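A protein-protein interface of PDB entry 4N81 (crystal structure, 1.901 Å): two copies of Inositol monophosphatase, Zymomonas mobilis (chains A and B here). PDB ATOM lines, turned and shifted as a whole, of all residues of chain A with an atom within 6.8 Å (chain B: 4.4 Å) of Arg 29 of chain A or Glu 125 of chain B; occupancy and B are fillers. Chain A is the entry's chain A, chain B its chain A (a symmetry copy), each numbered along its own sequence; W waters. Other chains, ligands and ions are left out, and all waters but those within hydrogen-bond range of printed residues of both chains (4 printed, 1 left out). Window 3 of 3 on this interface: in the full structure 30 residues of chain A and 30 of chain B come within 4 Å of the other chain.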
ATOM      1  N   ARG A  25       8.058  12.223 -10.784  1.00  0.00           N
ATOM      2  CA  ARG A  25       8.801  11.659 -11.930  1.00  0.00           C
ATOM      3  C   ARG A  25       9.063  10.133 -11.865  1.00  0.00           C
ATOM      4  O   ARG A  25       8.803   9.421 -12.841  1.00  0.00           O
ATOM      5  CB  ARG A  25      10.117  12.426 -12.109  1.00  0.00           C
ATOM      6  CG  ARG A  25      10.922  12.112 -13.360  1.00  0.00           C
ATOM      7  CD  ARG A  25      12.210  13.013 -13.423  1.00  0.00           C
ATOM      8  NE  ARG A  25      11.865  14.428 -13.628  1.00  0.00           N
ATOM      9  CZ  ARG A  25      12.011  15.376 -12.695  1.00  0.00           C
ATOM     10  NH1 ARG A  25      11.675  16.662 -12.964  1.00  0.00           N
ATOM     11  NH2 ARG A  25      12.504  15.047 -11.504  1.00  0.00           N
ATOM     12  N   PRO A  26       9.525   9.612 -10.710  1.00  0.00           N
ATOM     13  CA  PRO A  26       9.832   8.180 -10.656  1.00  0.00           C
ATOM     14  C   PRO A  26       8.604   7.304 -10.984  1.00  0.00           C
ATOM     15  O   PRO A  26       8.792   6.114 -11.257  1.00  0.00           O
ATOM     16  CB  PRO A  26      10.277   7.956  -9.197  1.00  0.00           C
ATOM     17  CG  PRO A  26      10.769   9.280  -8.755  1.00  0.00           C
ATOM     18  CD  PRO A  26       9.946  10.308  -9.478  1.00  0.00           C
ATOM     19  N   PHE A  27       7.383   7.809 -10.762  1.00  0.00           N
ATOM     20  CA  PHE A  27       6.172   7.001 -10.981  1.00  0.00           C
ATOM     21  C   PHE A  27       5.693   7.016 -12.426  1.00  0.00           C
ATOM     22  O   PHE A  27       4.826   6.258 -12.778  1.00  0.00           O
ATOM     23  CB  PHE A  27       5.029   7.484 -10.095  1.00  0.00           C
ATOM     24  CG  PHE A  27       5.298   7.273  -8.626  1.00  0.00           C
ATOM     25  CD1 PHE A  27       5.708   8.331  -7.812  1.00  0.00           C
ATOM     26  CD2 PHE A  27       5.215   6.004  -8.086  1.00  0.00           C
ATOM     27  CE1 PHE A  27       5.974   8.132  -6.472  1.00  0.00           C
ATOM     28  CE2 PHE A  27       5.485   5.788  -6.725  1.00  0.00           C
ATOM     29  CZ  PHE A  27       5.861   6.868  -5.925  1.00  0.00           C
ATOM     30  N   PHE A  28       6.211   7.919 -13.229  1.00  0.00           N
ATOM     31  CA  PHE A  28       5.720   8.033 -14.606  1.00  0.00           C
ATOM     32  C   PHE A  28       6.111   6.781 -15.415  1.00  0.00           C
ATOM     33  O   PHE A  28       7.283   6.351 -15.375  1.00  0.00           O
ATOM     34  CB  PHE A  28       6.336   9.287 -15.235  1.00  0.00           C
ATOM     35  CG  PHE A  28       5.882   9.515 -16.664  1.00  0.00           C
ATOM     36  CD1 PHE A  28       4.537   9.746 -16.935  1.00  0.00           C
ATOM     37  CD2 PHE A  28       6.817   9.532 -17.689  1.00  0.00           C
ATOM     38  CE1 PHE A  28       4.090   9.956 -18.270  1.00  0.00           C
ATOM     39  CE2 PHE A  28       6.431   9.781 -18.990  1.00  0.00           C
ATOM     40  CZ  PHE A  28       5.073  10.009 -19.284  1.00  0.00           C
ATOM     41  N   ARG A  29       5.156   6.247 -16.184  1.00  0.00           N
ATOM     42  CA  ARG A  29       5.379   5.032 -16.981  1.00  0.00           C
ATOM     43  C   ARG A  29       5.802   3.794 -16.196  1.00  0.00           C
ATOM     44  O   ARG A  29       6.396   2.868 -16.729  1.00  0.00           O
ATOM     45  CB  ARG A  29       6.364   5.310 -18.129  1.00  0.00           C
ATOM     46  CG  ARG A  29       5.653   6.113 -19.239  1.00  0.00           C
ATOM     47  CD  ARG A  29       6.538   6.380 -20.506  1.00  0.00           C
ATOM     48  NE  ARG A  29       5.800   7.290 -21.403  1.00  0.00           N
ATOM     49  CZ  ARG A  29       6.305   7.811 -22.527  1.00  0.00           C
ATOM     50  NH1 ARG A  29       7.538   7.485 -22.913  1.00  0.00           N
ATOM     51  NH2 ARG A  29       5.613   8.682 -23.219  1.00  0.00           N
ATOM     52  N   ALA A  30       5.442   3.770 -14.929  1.00  0.00           N
ATOM     53  CA  ALA A  30       5.531   2.572 -14.106  1.00  0.00           C
ATOM     54  C   ALA A  30       4.393   1.573 -14.467  1.00  0.00           C
ATOM     55  O   ALA A  30       3.346   1.954 -15.026  1.00  0.00           O
ATOM     56  CB  ALA A  30       5.466   2.959 -12.600  1.00  0.00           C
ATOM     57  N   PRO A  31       4.570   0.299 -14.112  1.00  0.00           N
ATOM     58  CA  PRO A  31       3.545  -0.733 -14.387  1.00  0.00           C
ATOM     59  C   PRO A  31       2.246  -0.413 -13.638  1.00  0.00           C
ATOM     60  O   PRO A  31       2.298   0.188 -12.571  1.00  0.00           O
ATOM     61  CB  PRO A  31       4.162  -2.015 -13.783  1.00  0.00           C
ATOM     62  CG  PRO A  31       5.619  -1.752 -13.750  1.00  0.00           C
ATOM     63  CD  PRO A  31       5.800  -0.263 -13.504  1.00  0.00           C
ATOM     64  N   PRO A  42       0.309   3.850  -9.370  1.00  0.00           N
ATOM     65  CA  PRO A  42       1.386   4.855  -9.280  1.00  0.00           C
ATOM     66  C   PRO A  42       0.872   6.298  -9.235  1.00  0.00           C
ATOM     67  O   PRO A  42       1.482   7.142  -8.541  1.00  0.00           O
ATOM     68  CB  PRO A  42       2.182   4.648 -10.587  1.00  0.00           C
ATOM     69  CG  PRO A  42       1.897   3.230 -10.992  1.00  0.00           C
ATOM     70  CD  PRO A  42       0.464   2.950 -10.533  1.00  0.00           C
ATOM     71  N   PHE A  94      -1.760  10.805 -17.428  1.00  0.00           N
ATOM     72  CA  PHE A  94      -0.614  10.242 -16.695  1.00  0.00           C
ATOM     73  C   PHE A  94      -0.740   8.721 -16.606  1.00  0.00           C
ATOM     74  O   PHE A  94       0.247   7.962 -16.804  1.00  0.00           O
ATOM     75  CB  PHE A  94      -0.590  10.814 -15.242  1.00  0.00           C
ATOM     76  CG  PHE A  94       0.551  10.275 -14.404  1.00  0.00           C
ATOM     77  CD1 PHE A  94       0.436   9.020 -13.787  1.00  0.00           C
ATOM     78  CD2 PHE A  94       1.707  10.996 -14.240  1.00  0.00           C
ATOM     79  CE1 PHE A  94       1.457   8.490 -13.016  1.00  0.00           C
ATOM     80  CE2 PHE A  94       2.766  10.486 -13.451  1.00  0.00           C
ATOM     81  CZ  PHE A  94       2.636   9.239 -12.836  1.00  0.00           C
ATOM     82  N   ILE A  95      -1.961   8.268 -16.368  1.00  0.00           N
ATOM     83  CA  ILE A  95      -2.198   6.822 -16.215  1.00  0.00           C
ATOM     84  C   ILE A  95      -1.877   6.122 -17.533  1.00  0.00           C
ATOM     85  O   ILE A  95      -1.310   5.004 -17.557  1.00  0.00           O
ATOM     86  CB  ILE A  95      -3.665   6.568 -15.820  1.00  0.00           C
ATOM     87  CG1 ILE A  95      -3.845   6.865 -14.319  1.00  0.00           C
ATOM     88  CG2 ILE A  95      -4.105   5.095 -16.090  1.00  0.00           C
ATOM     89  CD1 ILE A  95      -5.326   7.026 -13.922  1.00  0.00           C
ATOM     90  N   GLY A  96      -2.113   6.848 -18.620  1.00  0.00           N
ATOM     91  CA  GLY A  96      -1.819   6.322 -19.958  1.00  0.00           C
ATOM     92  C   GLY A  96      -0.372   6.520 -20.410  1.00  0.00           C
ATOM     93  O   GLY A  96      -0.013   6.207 -21.559  1.00  0.00           O
ATOM     94  N   GLY A  97       0.479   7.038 -19.522  1.00  0.00           N
ATOM     95  CA  GLY A  97       1.887   7.149 -19.885  1.00  0.00           C
ATOM     96  C   GLY A  97       2.190   8.338 -20.785  1.00  0.00           C
ATOM     97  O   GLY A  97       3.216   8.360 -21.478  1.00  0.00           O
ATOM     98  N   ARG A  98       1.263   9.306 -20.846  1.00  0.00           N
ATOM     99  CA  ARG A  98       1.473  10.521 -21.642  1.00  0.00           C
ATOM    100  C   ARG A  98       2.033  11.672 -20.861  1.00  0.00           C
ATOM    101  O   ARG A  98       1.561  11.957 -19.762  1.00  0.00           O
ATOM    102  CB  ARG A  98       0.135  11.029 -22.204  1.00  0.00           C
ATOM    103  CG  ARG A  98      -0.576   9.945 -23.106  1.00  0.00           C
ATOM    104  CD  ARG A  98      -1.950  10.528 -23.532  1.00  0.00           C
ATOM    105  NE  ARG A  98      -2.536   9.750 -24.651  1.00  0.00           N
ATOM    106  CZ  ARG A  98      -3.466  10.273 -25.452  1.00  0.00           C
ATOM    107  NH1 ARG A  98      -3.887  11.531 -25.244  1.00  0.00           N
ATOM    108  NH2 ARG A  98      -3.966   9.543 -26.445  1.00  0.00           N
ATOM    109  N   ALA A  99       2.977  12.396 -21.459  1.00  0.00           N
ATOM    110  CA  ALA A  99       3.595  13.520 -20.725  1.00  0.00           C
ATOM    111  C   ALA A  99       2.888  14.836 -21.069  1.00  0.00           C
ATOM    112  O   ALA A  99       3.534  15.885 -21.256  1.00  0.00           O
ATOM    113  CB  ALA A  99       5.084  13.612 -21.070  1.00  0.00           C
ATOM    114  N   ILE A 122       8.249  15.856 -16.707  1.00  0.00           N
ATOM    115  CA  ILE A 122       9.015  14.871 -17.483  1.00  0.00           C
ATOM    116  C   ILE A 122       9.873  15.611 -18.506  1.00  0.00           C
ATOM    117  O   ILE A 122      11.083  15.386 -18.607  1.00  0.00           O
ATOM    118  CB  ILE A 122       8.059  13.860 -18.211  1.00  0.00           C
ATOM    119  CG1 ILE A 122       7.074  13.252 -17.187  1.00  0.00           C
ATOM    120  CG2 ILE A 122       8.881  12.743 -18.951  1.00  0.00           C
ATOM    121  CD1 ILE A 122       7.748  12.649 -15.917  1.00  0.00           C
ATOM    122  N   HIS A 123       9.254  16.514 -19.253  1.00  0.00           N
ATOM    123  CA  HIS A 123      10.016  17.305 -20.253  1.00  0.00           C
ATOM    124  C   HIS A 123      10.544  18.637 -19.808  1.00  0.00           C
ATOM    125  O   HIS A 123      11.207  19.339 -20.577  1.00  0.00           O
ATOM    126  CB  HIS A 123       9.274  17.320 -21.582  1.00  0.00           C
ATOM    127  CG  HIS A 123       9.205  15.934 -22.159  1.00  0.00           C
ATOM    128  ND1 HIS A 123       8.029  15.344 -22.573  1.00  0.00           N
ATOM    129  CD2 HIS A 123      10.177  14.987 -22.278  1.00  0.00           C
ATOM    130  CE1 HIS A 123       8.288  14.107 -22.971  1.00  0.00           C
ATOM    131  NE2 HIS A 123       9.575  13.858 -22.781  1.00  0.00           N
ATOM    132  N   ILE B 118       9.178   4.061 -35.443  1.00  0.00           N
ATOM    133  CA  ILE B 118       8.511   5.319 -35.079  1.00  0.00           C
ATOM    134  C   ILE B 118       9.572   6.168 -34.407  1.00  0.00           C
ATOM    135  O   ILE B 118      10.177   5.730 -33.424  1.00  0.00           O
ATOM    136  CB  ILE B 118       7.387   5.140 -34.010  1.00  0.00           C
ATOM    137  CG1 ILE B 118       6.218   4.247 -34.538  1.00  0.00           C
ATOM    138  CG2 ILE B 118       6.837   6.517 -33.600  1.00  0.00           C
ATOM    139  CD1 ILE B 118       5.371   3.592 -33.342  1.00  0.00           C
ATOM    140  N   ASN B 119       9.770   7.397 -34.878  1.00  0.00           N
ATOM    141  CA  ASN B 119      10.727   8.258 -34.205  1.00  0.00           C
ATOM    142  C   ASN B 119      10.114   9.584 -33.841  1.00  0.00           C
ATOM    143  O   ASN B 119       9.635  10.294 -34.728  1.00  0.00           O
ATOM    144  CB  ASN B 119      11.946   8.528 -35.093  1.00  0.00           C
ATOM    145  CG  ASN B 119      13.054   9.281 -34.329  1.00  0.00           C
ATOM    146  OD1 ASN B 119      13.592   8.763 -33.368  1.00  0.00           O
ATOM    147  ND2 ASN B 119      13.363  10.516 -34.749  1.00  0.00           N
ATOM    148  N   GLN B 120      10.194   9.946 -32.561  1.00  0.00           N
ATOM    149  CA  GLN B 120       9.691  11.251 -32.116  1.00  0.00           C
ATOM    150  C   GLN B 120      10.946  12.077 -31.996  1.00  0.00           C
ATOM    151  O   GLN B 120      11.752  11.871 -31.074  1.00  0.00           O
ATOM    152  CB  GLN B 120       9.034  11.062 -30.713  1.00  0.00           C
ATOM    153  CG  GLN B 120       7.851  12.065 -30.496  1.00  0.00           C
ATOM    154  CD  GLN B 120       8.278  13.503 -30.785  1.00  0.00           C
ATOM    155  OE1 GLN B 120       9.258  13.992 -30.222  1.00  0.00           O
ATOM    156  NE2 GLN B 120       7.563  14.170 -31.665  1.00  0.00           N
ATOM    157  N   HIS B 123      11.491  14.690 -28.539  1.00  0.00           N
ATOM    158  CA  HIS B 123      11.915  14.028 -27.278  1.00  0.00           C
ATOM    159  C   HIS B 123      12.841  12.854 -27.404  1.00  0.00           C
ATOM    160  O   HIS B 123      13.255  12.269 -26.399  1.00  0.00           O
ATOM    161  CB  HIS B 123      10.710  13.801 -26.376  1.00  0.00           C
ATOM    162  CG  HIS B 123      10.125  15.116 -25.943  1.00  0.00           C
ATOM    163  ND1 HIS B 123       8.790  15.432 -26.081  1.00  0.00           N
ATOM    164  CD2 HIS B 123      10.743  16.235 -25.475  1.00  0.00           C
ATOM    165  CE1 HIS B 123       8.600  16.677 -25.667  1.00  0.00           C
ATOM    166  NE2 HIS B 123       9.769  17.193 -25.318  1.00  0.00           N
ATOM    167  N   GLN B 124      13.209  12.550 -28.643  1.00  0.00           N
ATOM    168  CA  GLN B 124      14.150  11.453 -28.921  1.00  0.00           C
ATOM    169  C   GLN B 124      13.639  10.126 -28.352  1.00  0.00           C
ATOM    170  O   GLN B 124      14.270   9.507 -27.495  1.00  0.00           O
ATOM    171  CB  GLN B 124      15.541  11.760 -28.355  1.00  0.00           C
ATOM    172  CG  GLN B 124      15.950  13.192 -28.525  1.00  0.00           C
ATOM    173  CD  GLN B 124      16.497  13.428 -29.868  1.00  0.00           C
ATOM    174  OE1 GLN B 124      15.879  13.059 -30.875  1.00  0.00           O
ATOM    175  NE2 GLN B 124      17.693  14.017 -29.919  1.00  0.00           N
ATOM    176  N   GLU B 125      12.483   9.713 -28.836  1.00  0.00           N
ATOM    177  CA  GLU B 125      11.925   8.435 -28.450  1.00  0.00           C
ATOM    178  C   GLU B 125      11.782   7.660 -29.753  1.00  0.00           C
ATOM    179  O   GLU B 125      11.078   8.112 -30.679  1.00  0.00           O
ATOM    180  CB  GLU B 125      10.528   8.676 -27.873  1.00  0.00           C
ATOM    181  CG  GLU B 125      10.576   9.627 -26.649  1.00  0.00           C
ATOM    182  CD  GLU B 125       9.180   9.883 -26.030  1.00  0.00           C
ATOM    183  OE1 GLU B 125       8.971   9.560 -24.828  1.00  0.00           O
ATOM    184  OE2 GLU B 125       8.323  10.427 -26.763  1.00  0.00           O
ATOM    185  N   ARG B 126      12.373   6.466 -29.785  1.00  0.00           N
ATOM    186  CA  ARG B 126      12.426   5.703 -31.015  1.00  0.00           C
ATOM    187  C   ARG B 126      12.044   4.239 -30.762  1.00  0.00           C
ATOM    188  O   ARG B 126      12.689   3.541 -29.949  1.00  0.00           O
ATOM    189  CB  ARG B 126      13.834   5.765 -31.628  1.00  0.00           C
ATOM    190  CG  ARG B 126      13.901   5.013 -32.980  1.00  0.00           C
ATOM    191  CD  ARG B 126      15.248   5.258 -33.731  1.00  0.00           C
ATOM    192  NE  ARG B 126      15.394   6.679 -34.042  1.00  0.00           N
ATOM    193  CZ  ARG B 126      16.401   7.217 -34.736  1.00  0.00           C
ATOM    194  NH1 ARG B 126      17.387   6.461 -35.231  1.00  0.00           N
ATOM    195  NH2 ARG B 126      16.411   8.531 -34.936  1.00  0.00           N
ATOM    196  N   TRP B 127      10.974   3.809 -31.427  1.00  0.00           N
ATOM    197  CA  TRP B 127      10.528   2.413 -31.400  1.00  0.00           C
ATOM    198  C   TRP B 127      11.046   1.721 -32.669  1.00  0.00           C
ATOM    199  O   TRP B 127      10.904   2.300 -33.744  1.00  0.00           O
ATOM    200  CB  TRP B 127       8.996   2.400 -31.507  1.00  0.00           C
ATOM    201  CG  TRP B 127       8.233   2.834 -30.284  1.00  0.00           C
ATOM    202  CD1 TRP B 127       7.669   1.995 -29.319  1.00  0.00           C
ATOM    203  CD2 TRP B 127       7.926   4.179 -29.889  1.00  0.00           C
ATOM    204  NE1 TRP B 127       7.062   2.776 -28.335  1.00  0.00           N
ATOM    205  CE2 TRP B 127       7.173   4.104 -28.677  1.00  0.00           C
ATOM    206  CE3 TRP B 127       8.240   5.449 -30.416  1.00  0.00           C
ATOM    207  CZ2 TRP B 127       6.663   5.258 -28.033  1.00  0.00           C
ATOM    208  CZ3 TRP B 127       7.748   6.594 -29.764  1.00  0.00           C
ATOM    209  CH2 TRP B 127       6.963   6.490 -28.588  1.00  0.00           C
ATOM    210  N   PHE B 137      12.659  -0.044 -27.604  1.00  0.00           N
ATOM    211  CA  PHE B 137      12.383   1.367 -27.477  1.00  0.00           C
ATOM    212  C   PHE B 137      13.661   1.984 -26.905  1.00  0.00           C
ATOM    213  O   PHE B 137      14.081   1.598 -25.820  1.00  0.00           O
ATOM    214  CB  PHE B 137      11.246   1.590 -26.516  1.00  0.00           C
ATOM    215  CG  PHE B 137      10.958   3.078 -26.248  1.00  0.00           C
ATOM    216  CD1 PHE B 137      11.416   3.694 -25.091  1.00  0.00           C
ATOM    217  CD2 PHE B 137      10.211   3.829 -27.162  1.00  0.00           C
ATOM    218  CE1 PHE B 137      11.115   5.076 -24.818  1.00  0.00           C
ATOM    219  CE2 PHE B 137       9.945   5.187 -26.937  1.00  0.00           C
ATOM    220  CZ  PHE B 137      10.391   5.817 -25.765  1.00  0.00           C
ATOM    221  N   ASN B 138      14.278   2.919 -27.636  1.00  0.00           N
ATOM    222  CA  ASN B 138      15.579   3.512 -27.214  1.00  0.00           C
ATOM    223  C   ASN B 138      16.554   2.411 -26.828  1.00  0.00           C
ATOM    224  O   ASN B 138      17.297   2.504 -25.843  1.00  0.00           O
ATOM    225  CB  ASN B 138      15.423   4.595 -26.137  1.00  0.00           C
ATOM    226  CG  ASN B 138      14.754   5.832 -26.690  1.00  0.00           C
ATOM    227  OD1 ASN B 138      14.589   5.931 -27.896  1.00  0.00           O
ATOM    228  ND2 ASN B 138      14.411   6.797 -25.836  1.00  0.00           N
ATOM    229  N   TYR B 188       1.571   7.741 -31.975  1.00  0.00           N
ATOM    230  CA  TYR B 188       2.104   7.697 -30.629  1.00  0.00           C
ATOM    231  C   TYR B 188       1.308   6.687 -29.793  1.00  0.00           C
ATOM    232  O   TYR B 188       1.890   6.019 -28.912  1.00  0.00           O
ATOM    233  CB  TYR B 188       2.015   9.086 -29.952  1.00  0.00           C
ATOM    234  CG  TYR B 188       3.090   9.230 -28.885  1.00  0.00           C
ATOM    235  CD1 TYR B 188       4.361   9.741 -29.205  1.00  0.00           C
ATOM    236  CD2 TYR B 188       2.839   8.879 -27.572  1.00  0.00           C
ATOM    237  CE1 TYR B 188       5.357   9.911 -28.222  1.00  0.00           C
ATOM    238  CE2 TYR B 188       3.837   9.011 -26.606  1.00  0.00           C
ATOM    239  CZ  TYR B 188       5.085   9.491 -26.929  1.00  0.00           C
ATOM    240  OH  TYR B 188       6.043   9.647 -25.919  1.00  0.00           O
ATOM    241  N   LEU B 192       2.611   3.727 -27.405  1.00  0.00           N
ATOM    242  CA  LEU B 192       2.358   3.556 -25.939  1.00  0.00           C
ATOM    243  C   LEU B 192       1.794   2.163 -25.724  1.00  0.00           C
ATOM    244  O   LEU B 192       2.038   1.508 -24.638  1.00  0.00           O
ATOM    245  CB  LEU B 192       1.311   4.620 -25.454  1.00  0.00           C
ATOM    246  CG  LEU B 192       1.929   6.026 -25.344  1.00  0.00           C
ATOM    247  CD1 LEU B 192       0.787   7.061 -25.096  1.00  0.00           C
ATOM    248  CD2 LEU B 192       3.004   6.045 -24.180  1.00  0.00           C
ATOM    249  N   HIS B 197       1.392   0.673 -21.988  1.00  0.00           N
ATOM    250  CA  HIS B 197       0.603   1.718 -21.282  1.00  0.00           C
ATOM    251  C   HIS B 197      -0.771   1.958 -21.883  1.00  0.00           C
ATOM    252  O   HIS B 197      -1.521   2.801 -21.390  1.00  0.00           O
ATOM    253  CB  HIS B 197       1.384   3.052 -21.324  1.00  0.00           C
ATOM    254  CG  HIS B 197       2.776   2.935 -20.794  1.00  0.00           C
ATOM    255  ND1 HIS B 197       3.044   2.477 -19.519  1.00  0.00           N
ATOM    256  CD2 HIS B 197       3.969   3.226 -21.354  1.00  0.00           C
ATOM    257  CE1 HIS B 197       4.355   2.471 -19.326  1.00  0.00           C
ATOM    258  NE2 HIS B 197       4.940   2.933 -20.423  1.00  0.00           N
HETATM  259  O   HOH W   1       4.201  11.417 -23.948  1.00  0.00           O
HETATM  260  O   HOH W   2      -1.822   5.133 -23.185  1.00  0.00           O
HETATM  261  O   HOH W   3      -1.879   2.642 -18.691  1.00  0.00           O
HETATM  262  O   HOH W   4       7.656  11.266 -23.192  1.00  0.00           O
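The side-chain hydroxyl of Tyr 188 of chain B lies within hydrogen-bond range of the guanidinium group of Arg 29 of chain A, 2.9 Å away.
The guanidinium group (NH1) of Arg 29 of chain A is in salt-bridge range of the side-chain carboxylate (OE1) of Glu 125 of chain B (3.2 Å).
The side-chain amide oxygen (OE1) of Gln 120 of chain B lies within hydrogen-bond range of the backbone NH (N) of His 123 of chain B, 2.9 Å away.
The backbone NH of His 197 of chain B sits at hydrogen-bond distance from the backbone carbonyl oxygen of Leu 192 of chain B.
The side-chain carboxylate of Glu 125 of chain B is in hydrogen-bond range of the side-chain hydroxyl of Tyr 188 of chain B (2.6 Å).
The backbone NH of Gln 120 of chain B is in hydrogen-bond range of the backbone carbonyl oxygen of Glu 125 of chain B (2.8 Å).
O of Gly 97 of chain A lies within hydrogen-bond range of NE of Arg 29 of chain A (2.8 Å).
Among the printed residues, pairs that only touch across the chains: Arg 29 of chain A with His 197 of chain B (3.3 Å), His 123 of chain A with His 123 of chain B (3.4 Å), Gly 96 of chain A with His 197 of chain B (3.5 Å), Gly 97 of chain A with Leu 192 of chain B (3.6 Å), Gly 96 of chain A with Leu 192 of chain B (3.7 Å), Arg 98 of chain A with Leu 192 of chain B (3.8 Å) and Arg 29 of chain A with Leu 192 of chain B (3.8 Å).
Of chain A, only Arg 29 (3.2 Å) comes within 4 Å of Glu 125 of chain B.
Of the printed residues of chain A, His 123 of chain B touches His 123 (3.4 Å).
Of the printed residues of chain B, His 123 of chain A touches His 123.
Of the printed residues of chain A, Tyr 188 of chain B touches Arg 29.
Of the printed residues of chain A, His 197 of chain B touches Arg 29 (3.3 Å) and Gly 96 (3.5 Å).
Of the printed residues of chain B, Gly 97 of chain A touches Leu 192.
Ala 99 of chain A touches none of the printed residues of chain B.
Phe 137 of chain B touches none of the printed residues of chain A.
Along chain B the printed residues that touch a printed residue of chain A span positions 123 to 197.
Of the 16 printed residues of chain A, 5 touch a printed residue of chain B.
Among the printed residues, Asp or Glu carboxylates within 4 Å of a Lys or Arg side-chain nitrogen of the other chain: Arg 29 of chain A with Glu 125 of chain B.
His 123 of chain B touches its own counterpart, His 123 of chain A.
1 position is printed for both chains.
Water W2 bridges the backbone carbonyl oxygen (O) of Gly 96 of chain A (2.7 Å) and the backbone carbonyl oxygen (O) of His 197 of chain B (3.0 Å).
Water W3 lies within hydrogen-bond range of the backbone carbonyl oxygen of Ile 95 of chain A (2.7 Å) and the backbone carbonyl oxygen of His 197 of chain B (2.7 Å).
Water W4 lies within hydrogen-bond range of OE1 of Glu 125 of chain B (2.7 Å), NE2 of His 123 of chain A (3.3 Å) and NH2 of Arg 29 of chain A (3.3 Å).
Water W1 lies within hydrogen-bond range of the backbone NH (N) of Ala 99 of chain A, the guanidinium group (NH2) of Arg 29 of chain A and the side-chain hydroxyl (OH) of Tyr 188 of chain B.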
